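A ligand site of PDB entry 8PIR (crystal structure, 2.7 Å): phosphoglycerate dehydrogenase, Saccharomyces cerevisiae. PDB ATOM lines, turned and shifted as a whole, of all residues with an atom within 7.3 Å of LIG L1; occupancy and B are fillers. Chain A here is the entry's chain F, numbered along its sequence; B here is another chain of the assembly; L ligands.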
ATOM      1  N   GLU A  69       9.422  16.850 -38.082  1.00  0.00           N
ATOM      2  CA  GLU A  69       9.603  17.473 -36.736  1.00  0.00           C
ATOM      3  C   GLU A  69      11.041  18.001 -36.598  1.00  0.00           C
ATOM      4  O   GLU A  69      11.500  18.211 -35.445  1.00  0.00           O
ATOM      5  CB  GLU A  69       9.265  16.477 -35.628  1.00  0.00           C
ATOM      6  CG  GLU A  69       7.783  16.359 -35.363  1.00  0.00           C
ATOM      7  CD  GLU A  69       7.379  15.126 -34.572  1.00  0.00           C
ATOM      8  OE1 GLU A  69       7.419  15.199 -33.334  1.00  0.00           O
ATOM      9  OE2 GLU A  69       7.012  14.114 -35.180  1.00  0.00           O
ATOM     10  N   ILE A 110      10.627  10.462 -36.925  1.00  0.00           N
ATOM     11  CA  ILE A 110       9.683  11.350 -36.190  1.00  0.00           C
ATOM     12  C   ILE A 110      10.361  11.828 -34.902  1.00  0.00           C
ATOM     13  O   ILE A 110      11.434  11.289 -34.554  1.00  0.00           O
ATOM     14  CB  ILE A 110       8.355  10.632 -35.902  1.00  0.00           C
ATOM     15  CG1 ILE A 110       8.508   9.534 -34.839  1.00  0.00           C
ATOM     16  CG2 ILE A 110       7.748  10.085 -37.186  1.00  0.00           C
ATOM     17  CD1 ILE A 110       7.195   8.910 -34.417  1.00  0.00           C
ATOM     18  N   ARG A 111       9.703  12.736 -34.189  1.00  0.00           N
ATOM     19  CA  ARG A 111       9.956  13.009 -32.745  1.00  0.00           C
ATOM     20  C   ARG A 111       8.665  12.711 -31.982  1.00  0.00           C
ATOM     21  O   ARG A 111       7.958  11.778 -32.397  1.00  0.00           O
ATOM     22  CB  ARG A 111      10.530  14.422 -32.598  1.00  0.00           C
ATOM     23  CG  ARG A 111      11.923  14.552 -33.212  1.00  0.00           C
ATOM     24  CD  ARG A 111      12.352  15.966 -33.467  1.00  0.00           C
ATOM     25  NE  ARG A 111      12.677  16.655 -32.236  1.00  0.00           N
ATOM     26  CZ  ARG A 111      13.298  17.831 -32.168  1.00  0.00           C
ATOM     27  NH1 ARG A 111      13.705  18.413 -33.280  1.00  0.00           N
ATOM     28  NH2 ARG A 111      13.522  18.413 -31.005  1.00  0.00           N
ATOM     29  N   SER A 112       8.428  13.393 -30.859  1.00  0.00           N
ATOM     30  CA  SER A 112       7.364  13.062 -29.874  1.00  0.00           C
ATOM     31  C   SER A 112       5.963  13.379 -30.426  1.00  0.00           C
ATOM     32  O   SER A 112       5.000  12.868 -29.842  1.00  0.00           O
ATOM     33  CB  SER A 112       7.603  13.770 -28.571  1.00  0.00           C
ATOM     34  OG  SER A 112       7.262  15.147 -28.686  1.00  0.00           O
ATOM     35  N   LYS A 113       5.848  14.234 -31.442  1.00  0.00           N
ATOM     36  CA  LYS A 113       4.552  14.831 -31.852  1.00  0.00           C
ATOM     37  C   LYS A 113       3.823  13.906 -32.839  1.00  0.00           C
ATOM     38  O   LYS A 113       2.635  13.622 -32.600  1.00  0.00           O
ATOM     39  CB  LYS A 113       4.747  16.243 -32.435  1.00  0.00           C
ATOM     40  CG  LYS A 113       4.822  17.342 -31.400  1.00  0.00           C
ATOM     41  CD  LYS A 113       5.149  18.708 -31.980  1.00  0.00           C
ATOM     42  CE  LYS A 113       5.582  19.704 -30.922  1.00  0.00           C
ATOM     43  NZ  LYS A 113       6.263  20.875 -31.522  1.00  0.00           N
ATOM     44  N   PHE A 133      13.601  10.010 -33.108  1.00  0.00           N
ATOM     45  CA  PHE A 133      14.760  10.899 -32.826  1.00  0.00           C
ATOM     46  C   PHE A 133      14.497  11.637 -31.515  1.00  0.00           C
ATOM     47  O   PHE A 133      14.416  12.879 -31.522  1.00  0.00           O
ATOM     48  CB  PHE A 133      15.001  11.853 -33.998  1.00  0.00           C
ATOM     49  CG  PHE A 133      15.540  11.165 -35.230  1.00  0.00           C
ATOM     50  CD1 PHE A 133      14.727  10.345 -35.994  1.00  0.00           C
ATOM     51  CD2 PHE A 133      16.888  11.227 -35.539  1.00  0.00           C
ATOM     52  CE1 PHE A 133      15.227   9.668 -37.091  1.00  0.00           C
ATOM     53  CE2 PHE A 133      17.401  10.516 -36.616  1.00  0.00           C
ATOM     54  CZ  PHE A 133      16.568   9.751 -37.395  1.00  0.00           C
ATOM     55  N   CYS A 134      14.461  10.874 -30.419  1.00  0.00           N
ATOM     56  CA  CYS A 134      13.949  11.268 -29.071  1.00  0.00           C
ATOM     57  C   CYS A 134      13.898  10.021 -28.185  1.00  0.00           C
ATOM     58  O   CYS A 134      14.270   8.949 -28.673  1.00  0.00           O
ATOM     59  CB  CYS A 134      12.568  11.900 -29.141  1.00  0.00           C
ATOM     60  SG  CYS A 134      11.311  10.814 -29.867  1.00  0.00           S
ATOM     61  N   ILE A 135      13.511  10.151 -26.926  1.00  0.00           N
ATOM     62  CA  ILE A 135      13.493   9.009 -25.966  1.00  0.00           C
ATOM     63  C   ILE A 135      12.164   8.270 -26.065  1.00  0.00           C
ATOM     64  O   ILE A 135      12.174   7.039 -25.990  1.00  0.00           O
ATOM     65  CB  ILE A 135      13.718   9.523 -24.534  1.00  0.00           C
ATOM     66  CG1 ILE A 135      14.933  10.446 -24.439  1.00  0.00           C
ATOM     67  CG2 ILE A 135      13.795   8.387 -23.537  1.00  0.00           C
ATOM     68  CD1 ILE A 135      15.124  11.036 -23.062  1.00  0.00           C
ATOM     69  N   GLY A 136      11.073   8.990 -26.282  1.00  0.00           N
ATOM     70  CA  GLY A 136       9.733   8.383 -26.296  1.00  0.00           C
ATOM     71  C   GLY A 136       9.406   7.543 -27.496  1.00  0.00           C
ATOM     72  O   GLY A 136       9.759   7.941 -28.592  1.00  0.00           O
ATOM     73  N   THR A 137       8.719   6.437 -27.275  1.00  0.00           N
ATOM     74  CA  THR A 137       8.247   5.559 -28.374  1.00  0.00           C
ATOM     75  C   THR A 137       6.724   5.381 -28.258  1.00  0.00           C
ATOM     76  O   THR A 137       6.198   4.560 -28.997  1.00  0.00           O
ATOM     77  CB  THR A 137       8.994   4.232 -28.303  1.00  0.00           C
ATOM     78  OG1 THR A 137       8.807   3.705 -26.985  1.00  0.00           O
ATOM     79  CG2 THR A 137      10.472   4.369 -28.572  1.00  0.00           C
ATOM     80  N   GLN A 139       4.252   7.459 -28.947  1.00  0.00           N
ATOM     81  CA  GLN A 139       3.585   8.081 -30.111  1.00  0.00           C
ATOM     82  C   GLN A 139       3.518   7.081 -31.276  1.00  0.00           C
ATOM     83  O   GLN A 139       2.925   7.413 -32.307  1.00  0.00           O
ATOM     84  CB  GLN A 139       4.295   9.373 -30.511  1.00  0.00           C
ATOM     85  CG  GLN A 139       5.646   9.161 -31.181  1.00  0.00           C
ATOM     86  CD  GLN A 139       6.784   9.042 -30.185  1.00  0.00           C
ATOM     87  OE1 GLN A 139       6.610   8.568 -29.074  1.00  0.00           O
ATOM     88  NE2 GLN A 139       7.967   9.440 -30.625  1.00  0.00           N
ATOM     89  N   SER A 155      16.639   7.003 -29.230  1.00  0.00           N
ATOM     90  CA  SER A 155      17.869   7.427 -28.510  1.00  0.00           C
ATOM     91  C   SER A 155      17.528   7.733 -27.052  1.00  0.00           C
ATOM     92  O   SER A 155      17.155   8.854 -26.723  1.00  0.00           O
ATOM     93  CB  SER A 155      18.539   8.626 -29.162  1.00  0.00           C
ATOM     94  N   PRO A 156      17.600   6.733 -26.142  1.00  0.00           N
ATOM     95  CA  PRO A 156      17.165   6.929 -24.769  1.00  0.00           C
ATOM     96  C   PRO A 156      18.097   7.792 -23.911  1.00  0.00           C
ATOM     97  O   PRO A 156      17.599   8.420 -23.001  1.00  0.00           O
ATOM     98  CB  PRO A 156      17.090   5.495 -24.202  1.00  0.00           C
ATOM     99  CG  PRO A 156      18.024   4.686 -25.092  1.00  0.00           C
ATOM    100  CD  PRO A 156      17.970   5.345 -26.446  1.00  0.00           C
ATOM    101  N   ASN A 159      20.999  12.368 -23.947  1.00  0.00           N
ATOM    102  CA  ASN A 159      20.597  13.673 -23.362  1.00  0.00           C
ATOM    103  C   ASN A 159      21.229  13.871 -21.978  1.00  0.00           C
ATOM    104  O   ASN A 159      20.951  14.916 -21.364  1.00  0.00           O
ATOM    105  CB  ASN A 159      19.075  13.796 -23.200  1.00  0.00           C
ATOM    106  CG  ASN A 159      18.378  14.166 -24.493  1.00  0.00           C
ATOM    107  OD1 ASN A 159      19.026  14.354 -25.522  1.00  0.00           O
ATOM    108  ND2 ASN A 159      17.078  14.345 -24.415  1.00  0.00           N
ATOM    109  N   HIS A 351      10.840  22.085 -20.127  1.00  0.00           N
ATOM    110  CA  HIS A 351      11.351  20.780 -20.615  1.00  0.00           C
ATOM    111  C   HIS A 351      12.568  20.985 -21.502  1.00  0.00           C
ATOM    112  O   HIS A 351      12.619  20.394 -22.568  1.00  0.00           O
ATOM    113  CB  HIS A 351      10.243  19.945 -21.274  1.00  0.00           C
ATOM    114  CG  HIS A 351      10.365  18.481 -21.027  1.00  0.00           C
ATOM    115  ND1 HIS A 351       9.272  17.695 -20.736  1.00  0.00           N
ATOM    116  CD2 HIS A 351      11.432  17.663 -21.010  1.00  0.00           C
ATOM    117  CE1 HIS A 351       9.657  16.453 -20.568  1.00  0.00           C
ATOM    118  NE2 HIS A 351      10.971  16.405 -20.724  1.00  0.00           N
ATOM    119  N   SER A 355      17.626  20.040 -24.270  1.00  0.00           N
ATOM    120  CA  SER A 355      17.444  20.995 -25.390  1.00  0.00           C
ATOM    121  C   SER A 355      18.769  21.729 -25.649  1.00  0.00           C
ATOM    122  O   SER A 355      18.861  22.924 -25.301  1.00  0.00           O
ATOM    123  CB  SER A 355      16.306  21.945 -25.117  1.00  0.00           C
ATOM    124  OG  SER A 355      15.063  21.239 -25.144  1.00  0.00           O
ATOM    125  N   GLN A 360      20.808  17.108 -29.675  1.00  0.00           N
ATOM    126  CA  GLN A 360      20.016  16.909 -30.915  1.00  0.00           C
ATOM    127  C   GLN A 360      20.898  16.257 -31.998  1.00  0.00           C
ATOM    128  O   GLN A 360      20.396  15.344 -32.705  1.00  0.00           O
ATOM    129  CB  GLN A 360      19.449  18.243 -31.415  1.00  0.00           C
ATOM    130  CG  GLN A 360      18.273  18.749 -30.598  1.00  0.00           C
ATOM    131  CD  GLN A 360      17.154  17.738 -30.557  1.00  0.00           C
ATOM    132  OE1 GLN A 360      16.492  17.471 -31.554  1.00  0.00           O
ATOM    133  NE2 GLN A 360      16.990  17.097 -29.408  1.00  0.00           N
ATOM    134  N   ILE A 363      21.644  12.589 -31.088  1.00  0.00           N
ATOM    135  CA  ILE A 363      20.371  11.870 -31.395  1.00  0.00           C
ATOM    136  C   ILE A 363      20.339  11.577 -32.891  1.00  0.00           C
ATOM    137  O   ILE A 363      20.102  10.413 -33.256  1.00  0.00           O
ATOM    138  CB  ILE A 363      19.143  12.689 -30.923  1.00  0.00           C
ATOM    139  CG1 ILE A 363      18.965  12.610 -29.414  1.00  0.00           C
ATOM    140  CG2 ILE A 363      17.879  12.246 -31.653  1.00  0.00           C
ATOM    141  CD1 ILE A 363      17.830  13.450 -28.876  1.00  0.00           C
ATOM    142  N   LYS B 192      10.145  26.040 -25.466  1.00  0.00           N
ATOM    143  CA  LYS B 192      11.176  24.965 -25.493  1.00  0.00           C
ATOM    144  C   LYS B 192      12.076  25.162 -26.718  1.00  0.00           C
ATOM    145  O   LYS B 192      11.647  24.813 -27.819  1.00  0.00           O
ATOM    146  CB  LYS B 192      10.486  23.595 -25.529  1.00  0.00           C
ATOM    147  CG  LYS B 192      11.410  22.396 -25.655  1.00  0.00           C
ATOM    148  CD  LYS B 192      10.662  21.085 -25.506  1.00  0.00           C
ATOM    149  CE  LYS B 192      11.564  19.871 -25.434  1.00  0.00           C
ATOM    150  NZ  LYS B 192      10.991  18.808 -24.569  1.00  0.00           N
HETATM  151  C1  LIG L   1      11.547  12.946 -25.680  1.00  0.00           C
HETATM  152  O1  LIG L   1      10.800  11.865 -25.777  1.00  0.00           O
HETATM  153  O2  LIG L   1      12.770  12.937 -25.670  1.00  0.00           O
HETATM  154  C2  LIG L   1      10.733  14.220 -25.553  1.00  0.00           C
HETATM  155  O3  LIG L   1       9.378  13.989 -25.937  1.00  0.00           O
HETATM  156  C3  LIG L   1      11.331  15.324 -26.392  1.00  0.00           C
HETATM  157  O4  LIG L   1      10.772  15.224 -27.718  1.00  0.00           O
HETATM  158  P1  LIG L   1      11.111  16.359 -28.813  1.00  0.00           P
HETATM  159  O5  LIG L   1       9.965  16.345 -29.837  1.00  0.00           O
HETATM  160  O6  LIG L   1      12.390  15.864 -29.526  1.00  0.00           O
HETATM  161  O7  LIG L   1      11.314  17.697 -28.140  1.00  0.00           O
HETATM  162  P1  LG2 L   2      18.143   5.661 -15.960  1.00  0.00           P
HETATM  163  O1  LG2 L   2      17.256   4.553 -16.291  1.00  0.00           O
HETATM  164  O2  LG2 L   2      19.629   5.568 -16.389  1.00  0.00           O
HETATM  165  O3  LG2 L   2      18.245   5.885 -14.362  1.00  0.00           O
HETATM  166  C1  LG2 L   2      17.082   5.802 -13.536  1.00  0.00           C
HETATM  167  C2  LG2 L   2      17.559   5.351 -12.176  1.00  0.00           C
HETATM  168  O4  LG2 L   2      16.453   5.416 -11.251  1.00  0.00           O
HETATM  169  C3  LG2 L   2      18.092   3.906 -12.118  1.00  0.00           C
HETATM  170  O5  LG2 L   2      19.359   3.884 -11.474  1.00  0.00           O
HETATM  171  C4  LG2 L   2      17.009   3.172 -11.301  1.00  0.00           C
HETATM  172  O6  LG2 L   2      17.501   2.118 -10.491  1.00  0.00           O
HETATM  173  C5  LG2 L   2      16.555   4.295 -10.399  1.00  0.00           C
HETATM  174  N1  LG2 L   2      15.276   4.092  -9.741  1.00  0.00           N
HETATM  175  C6  LG2 L   2      14.112   3.603 -10.286  1.00  0.00           C
HETATM  176  N2  LG2 L   2      13.074   3.705  -9.491  1.00  0.00           N
HETATM  177  C7  LG2 L   2      13.588   4.288  -8.345  1.00  0.00           C
HETATM  178  C8  LG2 L   2      12.968   4.799  -7.185  1.00  0.00           C
HETATM  179  N3  LG2 L   2      11.640   4.873  -7.038  1.00  0.00           N
HETATM  180  N4  LG2 L   2      13.741   5.441  -6.293  1.00  0.00           N
HETATM  181  C9  LG2 L   2      15.038   5.613  -6.572  1.00  0.00           C
HETATM  182  N5  LG2 L   2      15.718   5.197  -7.636  1.00  0.00           N
HETATM  183  C10 LG2 L   2      14.939   4.522  -8.482  1.00  0.00           C
HETATM  184  O7  LG2 L   2      17.514   7.033 -16.467  1.00  0.00           O
HETATM  185  P2  LG2 L   2      18.261   8.327 -17.037  1.00  0.00           P
HETATM  186  O8  LG2 L   2      18.545   8.027 -18.463  1.00  0.00           O
HETATM  187  O9  LG2 L   2      19.381   8.643 -16.139  1.00  0.00           O
HETATM  188  O10 LG2 L   2      17.135   9.466 -16.914  1.00  0.00           O
HETATM  189  C11 LG2 L   2      16.494   9.738 -15.632  1.00  0.00           C
HETATM  190  C12 LG2 L   2      15.100  10.310 -15.774  1.00  0.00           C
HETATM  191  O11 LG2 L   2      15.149  11.645 -16.349  1.00  0.00           O
HETATM  192  C13 LG2 L   2      14.145   9.530 -16.663  1.00  0.00           C
HETATM  193  O12 LG2 L   2      12.810   9.666 -16.171  1.00  0.00           O
HETATM  194  C14 LG2 L   2      14.286  10.261 -18.006  1.00  0.00           C
HETATM  195  O13 LG2 L   2      13.173  10.070 -18.864  1.00  0.00           O
HETATM  196  C15 LG2 L   2      14.370  11.704 -17.512  1.00  0.00           C
HETATM  197  N6  LG2 L   2      15.007  12.649 -18.498  1.00  0.00           N
HETATM  198  C16 LG2 L   2      14.463  13.876 -18.638  1.00  0.00           C
HETATM  199  C17 LG2 L   2      14.947  14.745 -19.597  1.00  0.00           C
HETATM  200  C18 LG2 L   2      14.565  16.189 -19.553  1.00  0.00           C
HETATM  201  O14 LG2 L   2      14.564  16.844 -20.584  1.00  0.00           O
HETATM  202  N7  LG2 L   2      14.231  16.708 -18.371  1.00  0.00           N
HETATM  203  C19 LG2 L   2      15.942  14.296 -20.470  1.00  0.00           C
HETATM  204  C20 LG2 L   2      16.491  13.036 -20.290  1.00  0.00           C
HETATM  205  C21 LG2 L   2      16.024  12.225 -19.268  1.00  0.00           C
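The guanidinium group of Arg 111 lies within salt-bridge range of an oxygen (O6) of LIG L1. An oxygen (O1) of LIG L1 is in hydrogen-bond range of the backbone NH (N) of Gly 136, at 2.9 Å. The backbone NH of Ile 135 lies within hydrogen-bond range of an oxygen (O2) of LIG L1. N of Ser 112 lies within hydrogen-bond range of O5 of LIG L1, 3.5 Å away. The side-chain hydroxyl (OG) of Ser 112 sits at hydrogen-bond distance from an oxygen (O5) of LIG L1, at 3.2 Å. The side-chain amino group of Lys 192 of chain B lies within salt-bridge range of an oxygen (O7) of LIG L1 (3.8 Å).
The backbone carbonyl oxygen (O) of Glu 69 is in hydrogen-bond range of the guanidinium group (NH1) of Arg 111 (3.1 Å). The guanidinium group (NH2) of Arg 111 is in hydrogen-bond range of the side-chain amide oxygen (OE1) of Gln 360. The backbone carbonyl oxygen of Arg 111 lies within hydrogen-bond range of the side-chain amide nitrogen of Gln 139. The side-chain amide nitrogen (NE2) of Gln 139 lies within hydrogen-bond range of the backbone carbonyl oxygen (O) of Gly 136, 3.1 Å away. The backbone NH (N) of Ser 112 is in hydrogen-bond range of the side-chain carboxylate (OE1) of Glu 69, at 3.2 Å. NZ of Lys 192 of chain B sits at hydrogen-bond distance from O of His 351 (3.0 Å). The backbone carbonyl oxygen (O) of Cys 134 sits at hydrogen-bond distance from the backbone NH (N) of Ser 155 (3.1 Å). SG of Cys 134 is in hydrogen-bond range of NE2 of Gln 139, at 3.7 Å.
Cys 134 touches LIG L1 (CB to O2, 3.6 Å). Hydrophobic or aromatic side chains that line LIG L1: Ile 135. Within 4 Å of LIG L1: Arg 111, Ser 112, Cys 134, Ile 135, Gly 136 and Lys 192 of chain B.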
